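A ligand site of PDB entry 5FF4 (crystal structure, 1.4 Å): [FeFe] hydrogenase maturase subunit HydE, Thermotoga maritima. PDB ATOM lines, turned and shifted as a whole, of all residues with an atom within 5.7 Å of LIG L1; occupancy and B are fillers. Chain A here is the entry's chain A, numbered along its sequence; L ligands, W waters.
The side-chain carboxylate (OE2) of Glu 171 sits at hydrogen-bond distance from an oxygen (O4) of LIG L1 (2.4 Å). N of Ile 241 sits at hydrogen-bond distance from N5 of LIG L1 (3.0 Å). O of Ile 241 is in hydrogen-bond range of N4 of LIG L1 (2.8 Å). O of Tyr 79 is in hydrogen-bond range of N4 of LIG L1 (2.9 Å). The guanidinium group (NH1) of Arg 169 sits at hydrogen-bond distance from an oxygen (O5) of LIG L1 (3.1 Å). An oxygen (O1) of LIG L1 lies within salt-bridge range of the guanidinium group (NH2) of Arg 190 (3.2 Å). O of Ser 118 sits close to N1 of LIG L1 (3.2 Å). An oxygen (O5) of LIG L1 sits close to the side-chain sulfur of Met 209 (3.8 Å). The side-chain sulfur (SG) of Cys 80 binds an iron atom (FE1) of LG2 L2. FE3 of LG2 L2 is bound by SG of Cys 73. The guanidinium group (NH2) of Arg 169 lies within salt-bridge range of an oxygen (O4) of LG3 L3, at 2.7 Å. O2 of LG3 L3 sits at hydrogen-bond distance from OH of Tyr 316, at 2.6 Å. The side-chain amide nitrogen (NE2) of Gln 117 lies close to a sulfur (S1) of LG3 L3, at 3.7 Å. The backbone NH (N) of Ala 280 is in hydrogen-bond range of an oxygen (O1) of LG3 L3, at 3.0 Å.
An oxygen (O2) of LIG L1 binds an iron atom (FE4) of LG2 L2 (2.2 Å).
The side-chain carboxylate (OE2) of Glu 171 lies within salt-bridge range of the guanidinium group (NH2) of Arg 190, 3.1 Å away. The backbone NH (N) of Met 209 sits at hydrogen-bond distance from the backbone carbonyl oxygen (O) of Glu 171 (3.2 Å). NE of Arg 182 lies within hydrogen-bond range of OH of Tyr 79 (3.1 Å). The backbone NH (N) of Ser 118 lies within hydrogen-bond range of the backbone carbonyl oxygen (O) of Ser 146 (3.3 Å). OE1 of Gln 117 lies within hydrogen-bond range of OH of Tyr 313 (3.2 Å). The backbone carbonyl oxygen (O) of Leu 315 is in hydrogen-bond range of the backbone NH (N) of Gly 81 (2.9 Å). The side-chain hydroxyl of Ser 146 is in hydrogen-bond range of the side-chain amide nitrogen of Gln 117 (3.2 Å). The backbone NH of Ala 280 sits at hydrogen-bond distance from the side-chain hydroxyl of Tyr 316 (3.2 Å).
CA of Cys 80 touches N3 of LIG L1, at 3.8 Å. Gln 117 touches LIG L1. O of Ser 146 touches C2 of LIG L1, at 3.6 Å. Gly 148 touches LIG L1 (N to C1, 3.8 Å). Leu 168 touches LIG L1 (CD1 to O1, 3.98 Å). Pro 239 touches LIG L1. Phe 240 touches LIG L1. Tyr 313 touches LIG L1 (OH to C3, 3.5 Å). Leu 315 touches LIG L1. CD2 of Tyr 316 touches C13 of LIG L1, at 3.7 Å. Hydrophobic or aromatic side chains within 4 Å of LIG L1: Tyr 79, Leu 168, Met 209, Ile 241, Leu 315 and Tyr 316. 17 residues have an atom within 4 Å of LIG L1: Tyr 79, Cys 80, Gln 117, Ser 118, Ser 146, Gly 148, Leu 168, Arg 169, Glu 171, Arg 190, Met 209, Pro 239, Phe 240, Ile 241, Tyr 313, Leu 315 and Tyr 316. Along chain A the residues within 4 Å of LIG L1 span positions 79 to 316.
Water W5 lies within hydrogen-bond range of an oxygen (O4) of LIG L1 and the backbone NH of Arg 169. Water W3 lies within hydrogen-bond range of the backbone carbonyl oxygen (O) of Leu 167 (2.7 Å), an oxygen (O1) of LIG L1 (2.7 Å), the side-chain hydroxyl (OG) of Ser 146 (2.9 Å), the backbone NH (N) of Gly 148 (3.0 Å) and the backbone NH (N) of Leu 147 (3.3 Å). Water W4 lies within hydrogen-bond range of N6 of LIG L1 (2.9 Å), O of Pro 239 (3.0 Å) and NH1 of Arg 169 (3.2 Å). Water W1 lies within hydrogen-bond range of the side-chain carboxylate (OE2) of Glu 120, the guanidinium group (NH1) of Arg 190 and the guanidinium group (NH2) of Arg 182. Water W2 lies within hydrogen-bond range of the side-chain carboxylate (OE2) of Glu 171 (2.7 Å), the side-chain hydroxyl (OH) of Tyr 79 (2.8 Å) and the guanidinium group (NE) of Arg 182 (3.1 Å).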
ATOM      1  N   CYS A  73      13.819   6.238  29.584  1.00  0.00           N
ATOM      2  CA  CYS A  73      13.155   6.488  28.335  1.00  0.00           C
ATOM      3  C   CYS A  73      12.051   5.512  27.990  1.00  0.00           C
ATOM      4  O   CYS A  73      12.235   4.319  28.182  1.00  0.00           O
ATOM      5  CB  CYS A  73      14.146   6.510  27.124  1.00  0.00           C
ATOM      6  SG  CYS A  73      13.418   7.334  25.679  1.00  0.00           S
ATOM      7  N   TYR A  79      19.156   2.662  17.667  1.00  0.00           N
ATOM      8  CA  TYR A  79      20.544   3.067  17.827  1.00  0.00           C
ATOM      9  C   TYR A  79      20.955   3.475  19.189  1.00  0.00           C
ATOM     10  O   TYR A  79      22.159   3.582  19.468  1.00  0.00           O
ATOM     11  CB  TYR A  79      20.781   4.243  16.901  1.00  0.00           C
ATOM     12  CG  TYR A  79      19.752   5.294  16.879  1.00  0.00           C
ATOM     13  CD1 TYR A  79      19.690   6.287  17.903  1.00  0.00           C
ATOM     14  CD2 TYR A  79      18.778   5.381  15.921  1.00  0.00           C
ATOM     15  CE1 TYR A  79      18.727   7.240  17.890  1.00  0.00           C
ATOM     16  CE2 TYR A  79      17.774   6.299  15.912  1.00  0.00           C
ATOM     17  CZ  TYR A  79      17.751   7.246  16.972  1.00  0.00           C
ATOM     18  OH  TYR A  79      16.766   8.160  16.951  1.00  0.00           O
ATOM     19  N   CYS A  80      20.041   3.653  20.104  1.00  0.00           N
ATOM     20  CA  CYS A  80      20.319   4.405  21.359  1.00  0.00           C
ATOM     21  C   CYS A  80      20.543   3.541  22.559  1.00  0.00           C
ATOM     22  O   CYS A  80      19.650   2.690  22.860  1.00  0.00           O
ATOM     23  CB  CYS A  80      19.167   5.320  21.660  1.00  0.00           C
ATOM     24  SG  CYS A  80      19.434   6.420  23.051  1.00  0.00           S
ATOM     25  N   GLY A  81      21.581   3.752  23.346  1.00  0.00           N
ATOM     26  CA  GLY A  81      21.777   3.042  24.545  1.00  0.00           C
ATOM     27  C   GLY A  81      20.774   3.210  25.661  1.00  0.00           C
ATOM     28  O   GLY A  81      20.702   2.389  26.575  1.00  0.00           O
ATOM     29  N   GLN A 117      18.530  17.968  29.146  1.00  0.00           N
ATOM     30  CA  GLN A 117      18.352  16.860  28.245  1.00  0.00           C
ATOM     31  C   GLN A 117      18.018  15.593  29.024  1.00  0.00           C
ATOM     32  O   GLN A 117      18.564  15.372  30.086  1.00  0.00           O
ATOM     33  CB  GLN A 117      19.567  16.626  27.329  1.00  0.00           C
ATOM     34  CG  GLN A 117      19.321  15.658  26.193  1.00  0.00           C
ATOM     35  CD  GLN A 117      20.456  15.492  25.266  1.00  0.00           C
ATOM     36  OE1 GLN A 117      21.414  14.740  25.631  1.00  0.00           O
ATOM     37  NE2 GLN A 117      20.458  16.056  24.146  1.00  0.00           N
ATOM     38  N   SER A 118      17.147  14.779  28.452  1.00  0.00           N
ATOM     39  CA  SER A 118      16.792  13.538  29.088  1.00  0.00           C
ATOM     40  C   SER A 118      16.321  12.559  28.049  1.00  0.00           C
ATOM     41  O   SER A 118      15.980  12.879  26.923  1.00  0.00           O
ATOM     42  CB  SER A 118      15.713  13.719  30.157  1.00  0.00           C
ATOM     43  OG  SER A 118      14.527  14.255  29.578  1.00  0.00           O
ATOM     44  N   GLY A 119      16.229  11.288  28.517  1.00  0.00           N
ATOM     45  CA  GLY A 119      15.350  10.322  27.837  1.00  0.00           C
ATOM     46  C   GLY A 119      13.910  10.850  27.875  1.00  0.00           C
ATOM     47  O   GLY A 119      13.586  11.798  28.629  1.00  0.00           O
ATOM     48  N   GLU A 120      13.038  10.298  27.102  1.00  0.00           N
ATOM     49  CA  GLU A 120      11.615  10.610  27.210  1.00  0.00           C
ATOM     50  C   GLU A 120      11.069   9.973  28.444  1.00  0.00           C
ATOM     51  O   GLU A 120      10.459   8.847  28.407  1.00  0.00           O
ATOM     52  CB  GLU A 120      10.830  10.169  25.972  1.00  0.00           C
ATOM     53  CG  GLU A 120      11.182  10.970  24.736  1.00  0.00           C
ATOM     54  CD  GLU A 120      10.203  10.789  23.577  1.00  0.00           C
ATOM     55  OE1 GLU A 120       9.172  10.108  23.793  1.00  0.00           O
ATOM     56  OE2 GLU A 120      10.481  11.307  22.472  1.00  0.00           O
ATOM     57  N   SER A 146      15.757  19.616  25.689  1.00  0.00           N
ATOM     58  CA  SER A 146      15.928  18.552  24.681  1.00  0.00           C
ATOM     59  C   SER A 146      15.371  17.288  25.328  1.00  0.00           C
ATOM     60  O   SER A 146      16.080  16.441  25.846  1.00  0.00           O
ATOM     61  CB  SER A 146      17.422  18.403  24.414  1.00  0.00           C
ATOM     62  OG  SER A 146      17.695  17.396  23.421  1.00  0.00           O
ATOM     63  N   LEU A 147      14.032  17.191  25.291  1.00  0.00           N
ATOM     64  CA  LEU A 147      13.269  16.191  26.038  1.00  0.00           C
ATOM     65  C   LEU A 147      12.543  15.211  25.105  1.00  0.00           C
ATOM     66  O   LEU A 147      11.863  14.316  25.603  1.00  0.00           O
ATOM     67  CB  LEU A 147      12.282  16.822  26.982  1.00  0.00           C
ATOM     68  CG  LEU A 147      12.806  17.970  27.824  1.00  0.00           C
ATOM     69  CD1 LEU A 147      11.735  18.548  28.729  1.00  0.00           C
ATOM     70  CD2 LEU A 147      14.015  17.560  28.644  1.00  0.00           C
ATOM     71  N   GLY A 148      12.719  15.333  23.772  1.00  0.00           N
ATOM     72  CA  GLY A 148      12.015  14.443  22.845  1.00  0.00           C
ATOM     73  C   GLY A 148      10.647  14.979  22.420  1.00  0.00           C
ATOM     74  O   GLY A 148      10.367  16.176  22.421  1.00  0.00           O
ATOM     75  N   LEU A 167      15.865  21.538  21.292  1.00  0.00           N
ATOM     76  CA  LEU A 167      16.622  20.706  20.396  1.00  0.00           C
ATOM     77  C   LEU A 167      15.849  19.445  20.136  1.00  0.00           C
ATOM     78  O   LEU A 167      15.531  18.694  21.074  1.00  0.00           O
ATOM     79  CB  LEU A 167      17.971  20.329  20.995  1.00  0.00           C
ATOM     80  CG  LEU A 167      18.797  21.547  21.520  1.00  0.00           C
ATOM     81  CD1 LEU A 167      20.039  20.896  22.257  1.00  0.00           C
ATOM     82  CD2 LEU A 167      19.075  22.581  20.406  1.00  0.00           C
ATOM     83  N   LEU A 168      15.603  19.158  18.853  1.00  0.00           N
ATOM     84  CA  LEU A 168      14.887  17.914  18.449  1.00  0.00           C
ATOM     85  C   LEU A 168      15.482  17.491  17.094  1.00  0.00           C
ATOM     86  O   LEU A 168      14.960  17.865  16.046  1.00  0.00           O
ATOM     87  CB  LEU A 168      13.383  18.152  18.385  1.00  0.00           C
ATOM     88  CG  LEU A 168      12.598  16.864  18.336  1.00  0.00           C
ATOM     89  CD1 LEU A 168      12.606  16.090  19.648  1.00  0.00           C
ATOM     90  CD2 LEU A 168      11.120  17.146  17.944  1.00  0.00           C
ATOM     91  N   ARG A 169      16.572  16.786  17.110  1.00  0.00           N
ATOM     92  CA  ARG A 169      17.185  16.375  15.839  1.00  0.00           C
ATOM     93  C   ARG A 169      16.182  15.612  15.028  1.00  0.00           C
ATOM     94  O   ARG A 169      15.428  14.793  15.511  1.00  0.00           O
ATOM     95  CB  ARG A 169      18.347  15.459  16.103  1.00  0.00           C
ATOM     96  CG  ARG A 169      19.559  16.234  16.623  1.00  0.00           C
ATOM     97  CD  ARG A 169      20.598  15.129  16.855  1.00  0.00           C
ATOM     98  NE  ARG A 169      21.807  15.767  17.252  1.00  0.00           N
ATOM     99  CZ  ARG A 169      22.997  15.151  17.093  1.00  0.00           C
ATOM    100  NH1 ARG A 169      23.037  13.849  16.655  1.00  0.00           N
ATOM    101  NH2 ARG A 169      24.047  15.793  17.366  1.00  0.00           N
ATOM    102  N   GLU A 171      17.043  13.411  12.894  1.00  0.00           N
ATOM    103  CA  GLU A 171      17.679  12.102  12.894  1.00  0.00           C
ATOM    104  C   GLU A 171      18.029  11.582  11.463  1.00  0.00           C
ATOM    105  O   GLU A 171      19.211  11.320  11.223  1.00  0.00           O
ATOM    106  CB  GLU A 171      16.897  11.018  13.680  1.00  0.00           C
ATOM    107  CG  GLU A 171      16.493  11.474  15.089  1.00  0.00           C
ATOM    108  CD  GLU A 171      17.590  11.792  16.036  1.00  0.00           C
ATOM    109  OE1 GLU A 171      18.738  11.797  15.676  1.00  0.00           O
ATOM    110  OE2 GLU A 171      17.188  12.061  17.212  1.00  0.00           O
ATOM    111  N   ARG A 182      13.174   4.084  14.479  1.00  0.00           N
ATOM    112  CA  ARG A 182      12.429   4.719  15.600  1.00  0.00           C
ATOM    113  C   ARG A 182      10.996   4.186  15.569  1.00  0.00           C
ATOM    114  O   ARG A 182      10.072   4.846  15.126  1.00  0.00           O
ATOM    115  CB  ARG A 182      12.486   6.228  15.407  1.00  0.00           C
ATOM    116  CG  ARG A 182      13.920   6.737  15.236  1.00  0.00           C
ATOM    117  CD  ARG A 182      14.065   8.245  15.284  1.00  0.00           C
ATOM    118  NE  ARG A 182      13.756   8.739  16.654  1.00  0.00           N
ATOM    119  CZ  ARG A 182      12.707   9.432  16.957  1.00  0.00           C
ATOM    120  NH1 ARG A 182      11.926  10.000  16.117  1.00  0.00           N
ATOM    121  NH2 ARG A 182      12.504   9.570  18.309  1.00  0.00           N
ATOM    122  N   ARG A 190       7.956  13.657  13.898  1.00  0.00           N
ATOM    123  CA  ARG A 190       9.135  14.436  14.237  1.00  0.00           C
ATOM    124  C   ARG A 190       9.077  15.805  13.672  1.00  0.00           C
ATOM    125  O   ARG A 190       9.330  16.830  14.337  1.00  0.00           O
ATOM    126  CB  ARG A 190      10.368  13.649  13.795  1.00  0.00           C
ATOM    127  CG  ARG A 190      11.710  14.073  14.401  1.00  0.00           C
ATOM    128  CD  ARG A 190      11.751  13.590  15.859  1.00  0.00           C
ATOM    129  NE  ARG A 190      13.112  13.696  16.418  1.00  0.00           N
ATOM    130  CZ  ARG A 190      13.378  13.408  17.686  1.00  0.00           C
ATOM    131  NH1 ARG A 190      12.509  12.849  18.448  1.00  0.00           N
ATOM    132  NH2 ARG A 190      14.617  13.632  18.117  1.00  0.00           N
ATOM    133  N   SER A 208      20.969  15.607  12.489  1.00  0.00           N
ATOM    134  CA  SER A 208      20.910  14.234  12.035  1.00  0.00           C
ATOM    135  C   SER A 208      22.149  13.519  12.384  1.00  0.00           C
ATOM    136  O   SER A 208      23.212  14.111  12.675  1.00  0.00           O
ATOM    137  CB  SER A 208      20.632  14.163  10.515  1.00  0.00           C
ATOM    138  OG  SER A 208      21.497  14.976   9.793  1.00  0.00           O
ATOM    139  N   MET A 209      22.055  12.182  12.344  1.00  0.00           N
ATOM    140  CA  MET A 209      23.247  11.335  12.490  1.00  0.00           C
ATOM    141  C   MET A 209      23.733  10.965  11.048  1.00  0.00           C
ATOM    142  O   MET A 209      22.977  10.920  10.086  1.00  0.00           O
ATOM    143  CB  MET A 209      22.992  10.053  13.230  1.00  0.00           C
ATOM    144  CG  MET A 209      22.784  10.296  14.735  1.00  0.00           C
ATOM    145  SD  MET A 209      22.236   8.817  15.648  1.00  0.00           S
ATOM    146  CE  MET A 209      20.568   8.860  15.186  1.00  0.00           C
ATOM    147  N   PRO A 239      28.279  11.718  14.159  1.00  0.00           N
ATOM    148  CA  PRO A 239      28.238  10.332  13.610  1.00  0.00           C
ATOM    149  C   PRO A 239      27.335   9.464  14.442  1.00  0.00           C
ATOM    150  O   PRO A 239      27.131   9.706  15.599  1.00  0.00           O
ATOM    151  CB  PRO A 239      29.668   9.875  13.814  1.00  0.00           C
ATOM    152  CG  PRO A 239      30.137  10.528  15.045  1.00  0.00           C
ATOM    153  CD  PRO A 239      29.603  11.912  14.869  1.00  0.00           C
ATOM    154  N   PHE A 240      26.815   8.421  13.795  1.00  0.00           N
ATOM    155  CA  PHE A 240      26.237   7.285  14.511  1.00  0.00           C
ATOM    156  C   PHE A 240      27.401   6.495  15.102  1.00  0.00           C
ATOM    157  O   PHE A 240      28.372   6.194  14.476  1.00  0.00           O
ATOM    158  CB  PHE A 240      25.478   6.391  13.500  1.00  0.00           C
ATOM    159  CG  PHE A 240      25.193   5.031  14.013  1.00  0.00           C
ATOM    160  CD1 PHE A 240      24.373   4.799  15.087  1.00  0.00           C
ATOM    161  CD2 PHE A 240      25.789   3.945  13.374  1.00  0.00           C
ATOM    162  CE1 PHE A 240      24.149   3.516  15.545  1.00  0.00           C
ATOM    163  CE2 PHE A 240      25.536   2.648  13.876  1.00  0.00           C
ATOM    164  CZ  PHE A 240      24.726   2.469  14.941  1.00  0.00           C
ATOM    165  N   ILE A 241      27.260   6.152  16.373  1.00  0.00           N
ATOM    166  CA  ILE A 241      28.275   5.384  17.071  1.00  0.00           C
ATOM    167  C   ILE A 241      27.545   4.133  17.652  1.00  0.00           C
ATOM    168  O   ILE A 241      26.662   4.260  18.549  1.00  0.00           O
ATOM    169  CB  ILE A 241      28.906   6.195  18.203  1.00  0.00           C
ATOM    170  CG1 ILE A 241      29.684   7.403  17.617  1.00  0.00           C
ATOM    171  CG2 ILE A 241      29.896   5.340  18.980  1.00  0.00           C
ATOM    172  CD1 ILE A 241      30.211   8.363  18.632  1.00  0.00           C
ATOM    173  N   PRO A 242      27.873   2.921  17.156  1.00  0.00           N
ATOM    174  CA  PRO A 242      27.128   1.752  17.647  1.00  0.00           C
ATOM    175  C   PRO A 242      27.312   1.517  19.133  1.00  0.00           C
ATOM    176  O   PRO A 242      28.376   1.623  19.681  1.00  0.00           O
ATOM    177  CB  PRO A 242      27.735   0.614  16.814  1.00  0.00           C
ATOM    178  CG  PRO A 242      29.142   1.062  16.519  1.00  0.00           C
ATOM    179  CD  PRO A 242      29.054   2.562  16.337  1.00  0.00           C
ATOM    180  N   HIS A 243      26.195   1.095  19.751  1.00  0.00           N
ATOM    181  CA  HIS A 243      26.168   0.847  21.171  1.00  0.00           C
ATOM    182  C   HIS A 243      25.962  -0.712  21.355  1.00  0.00           C
ATOM    183  O   HIS A 243      25.058  -1.292  20.735  1.00  0.00           O
ATOM    184  CB  HIS A 243      25.038   1.622  21.845  1.00  0.00           C
ATOM    185  CG  HIS A 243      25.058   1.549  23.336  1.00  0.00           C
ATOM    186  ND1 HIS A 243      24.860   0.363  24.058  1.00  0.00           N
ATOM    187  CD2 HIS A 243      25.241   2.527  24.261  1.00  0.00           C
ATOM    188  CE1 HIS A 243      24.892   0.633  25.324  1.00  0.00           C
ATOM    189  NE2 HIS A 243      25.134   1.928  25.473  1.00  0.00           N
ATOM    190  N   ALA A 280      29.881  13.758  20.128  1.00  0.00           N
ATOM    191  CA  ALA A 280      30.089  12.554  19.280  1.00  0.00           C
ATOM    192  C   ALA A 280      31.260  12.711  18.316  1.00  0.00           C
ATOM    193  O   ALA A 280      31.999  11.776  18.175  1.00  0.00           O
ATOM    194  CB  ALA A 280      28.794  12.202  18.557  1.00  0.00           C
ATOM    195  N   TYR A 313      24.691   8.002  31.586  1.00  0.00           N
ATOM    196  CA  TYR A 313      23.988   8.569  30.446  1.00  0.00           C
ATOM    197  C   TYR A 313      24.711   8.211  29.161  1.00  0.00           C
ATOM    198  O   TYR A 313      25.441   8.982  28.587  1.00  0.00           O
ATOM    199  CB  TYR A 313      23.796  10.054  30.521  1.00  0.00           C
ATOM    200  CG  TYR A 313      22.721  10.618  29.609  1.00  0.00           C
ATOM    201  CD1 TYR A 313      21.413  10.670  29.937  1.00  0.00           C
ATOM    202  CD2 TYR A 313      23.060  11.109  28.382  1.00  0.00           C
ATOM    203  CE1 TYR A 313      20.458  11.252  29.149  1.00  0.00           C
ATOM    204  CE2 TYR A 313      22.116  11.693  27.586  1.00  0.00           C
ATOM    205  CZ  TYR A 313      20.865  11.708  27.964  1.00  0.00           C
ATOM    206  OH  TYR A 313      19.940  12.288  27.155  1.00  0.00           O
ATOM    207  N   LEU A 315      24.225   7.263  25.607  1.00  0.00           N
ATOM    208  CA  LEU A 315      23.559   7.074  24.401  1.00  0.00           C
ATOM    209  C   LEU A 315      24.432   6.233  23.443  1.00  0.00           C
ATOM    210  O   LEU A 315      23.863   5.421  22.747  1.00  0.00           O
ATOM    211  CB  LEU A 315      23.320   8.470  23.761  1.00  0.00           C
ATOM    212  CG  LEU A 315      22.573   9.443  24.596  1.00  0.00           C
ATOM    213  CD1 LEU A 315      22.738  10.810  23.899  1.00  0.00           C
ATOM    214  CD2 LEU A 315      21.138   9.090  24.666  1.00  0.00           C
ATOM    215  N   TYR A 316      25.770   6.397  23.550  1.00  0.00           N
ATOM    216  CA  TYR A 316      26.713   5.700  22.768  1.00  0.00           C
ATOM    217  C   TYR A 316      27.936   5.498  23.630  1.00  0.00           C
ATOM    218  O   TYR A 316      28.120   6.267  24.588  1.00  0.00           O
ATOM    219  CB  TYR A 316      27.000   6.479  21.504  1.00  0.00           C
ATOM    220  CG  TYR A 316      27.388   7.923  21.684  1.00  0.00           C
ATOM    221  CD1 TYR A 316      28.684   8.270  22.013  1.00  0.00           C
ATOM    222  CD2 TYR A 316      26.471   8.927  21.532  1.00  0.00           C
ATOM    223  CE1 TYR A 316      29.048   9.586  22.237  1.00  0.00           C
ATOM    224  CE2 TYR A 316      26.840  10.258  21.741  1.00  0.00           C
ATOM    225  CZ  TYR A 316      28.115  10.553  22.038  1.00  0.00           C
ATOM    226  OH  TYR A 316      28.503  11.866  22.259  1.00  0.00           O
HETATM  227  N1  LIG L   1      15.472  11.753  23.938  1.00  0.00           N
HETATM  228  C1  LIG L   1      15.724  13.099  23.317  1.00  0.00           C
HETATM  229  C2  LIG L   1      17.079  13.581  23.817  1.00  0.00           C
HETATM  230  C3  LIG L   1      18.231  12.605  24.101  1.00  0.00           C
HETATM  231  S1  LIG L   1      18.852  11.709  22.690  1.00  0.00           S
HETATM  232  C4  LIG L   1      15.682  12.866  21.865  1.00  0.00           C
HETATM  233  O1  LIG L   1      15.585  13.916  21.136  1.00  0.00           O
HETATM  234  O2  LIG L   1      15.668  11.691  21.326  1.00  0.00           O
HETATM  235  C5  LIG L   1      19.712  13.038  21.832  1.00  0.00           C
HETATM  236  C6  LIG L   1      20.360  12.615  20.491  1.00  0.00           C
HETATM  237  O3  LIG L   1      21.341  11.554  20.686  1.00  0.00           O
HETATM  238  C7  LIG L   1      19.480  12.006  19.428  1.00  0.00           C
HETATM  239  O4  LIG L   1      18.757  13.038  18.769  1.00  0.00           O
HETATM  240  C8  LIG L   1      20.445  11.199  18.504  1.00  0.00           C
HETATM  241  O5  LIG L   1      20.792  11.869  17.301  1.00  0.00           O
HETATM  242  C9  LIG L   1      21.715  11.030  19.395  1.00  0.00           C
HETATM  243  N2  LIG L   1      22.118   9.689  19.606  1.00  0.00           N
HETATM  244  C10 LIG L   1      21.385   8.731  20.200  1.00  0.00           C
HETATM  245  N3  LIG L   1      22.023   7.514  20.100  1.00  0.00           N
HETATM  246  C11 LIG L   1      23.187   7.729  19.352  1.00  0.00           C
HETATM  247  C12 LIG L   1      24.237   6.905  18.947  1.00  0.00           C
HETATM  248  N4  LIG L   1      24.233   5.591  19.145  1.00  0.00           N
HETATM  249  N5  LIG L   1      25.232   7.474  18.211  1.00  0.00           N
HETATM  250  C13 LIG L   1      25.311   8.819  18.046  1.00  0.00           C
HETATM  251  N6  LIG L   1      24.301   9.657  18.425  1.00  0.00           N
HETATM  252  C14 LIG L   1      23.275   9.159  19.107  1.00  0.00           C
HETATM  253 SE1  LG2 L   2      15.699   5.756  22.950  1.00  0.00          SE
HETATM  254 FE1  LG2 L   2      17.402   7.467  23.009  1.00  0.00          FE
HETATM  255 FE2  LG2 L   2      15.254   7.464  21.299  1.00  0.00          FE
HETATM  256 FE3  LG2 L   2      14.976   7.675  24.089  1.00  0.00          FE
HETATM  257 SE2  LG2 L   2      16.898   8.862  24.767  1.00  0.00          SE
HETATM  258 FE4  LG2 L   2      16.064  10.005  22.699  1.00  0.00          FE
HETATM  259 SE3  LG2 L   2      17.276   8.713  20.981  1.00  0.00          SE
HETATM  260 SE4  LG2 L   2      13.783   8.986  22.436  1.00  0.00          SE
HETATM  261  C1  LG3 L   3      23.952  17.357  21.175  1.00  0.00           C
HETATM  262  C2  LG3 L   3      25.269  15.445  21.735  1.00  0.00           C
HETATM  263  C3  LG3 L   3      23.958  14.697  21.516  1.00  0.00           C
HETATM  264  S1  LG3 L   3      22.714  15.982  21.218  1.00  0.00           S
HETATM  265  O1  LG3 L   3      27.072  14.619  20.427  1.00  0.00           O
HETATM  266  C4  LG3 L   3      26.477  14.564  21.504  1.00  0.00           C
HETATM  267  O2  LG3 L   3      26.790  13.813  22.451  1.00  0.00           O
HETATM  268  N1  LG3 L   3      25.230  16.706  20.972  1.00  0.00           N
HETATM  269  C5  LG3 L   3      23.913  18.049  22.517  1.00  0.00           C
HETATM  270  C6  LG3 L   3      23.686  18.290  20.023  1.00  0.00           C
HETATM  271  O3  LG3 L   3      22.844  19.193  20.207  1.00  0.00           O
HETATM  272  O4  LG3 L   3      24.121  17.965  18.934  1.00  0.00           O
HETATM  273  C7  LG3 L   3      23.544  13.888  22.708  1.00  0.00           C
HETATM  274  C8  LG3 L   3      24.062  13.765  20.260  1.00  0.00           C
HETATM  275  O   HOH W   1      12.670  11.694  20.974  1.00  0.00           O
HETATM  276  O   HOH W   2      15.693  10.209  18.573  1.00  0.00           O
HETATM  277  O   HOH W   3      15.226  16.350  22.364  1.00  0.00           O
HETATM  278  O   HOH W   4      25.448  11.815  16.945  1.00  0.00           O
HETATM  279  O   HOH W   5      17.396  15.241  19.534  1.00  0.00           O
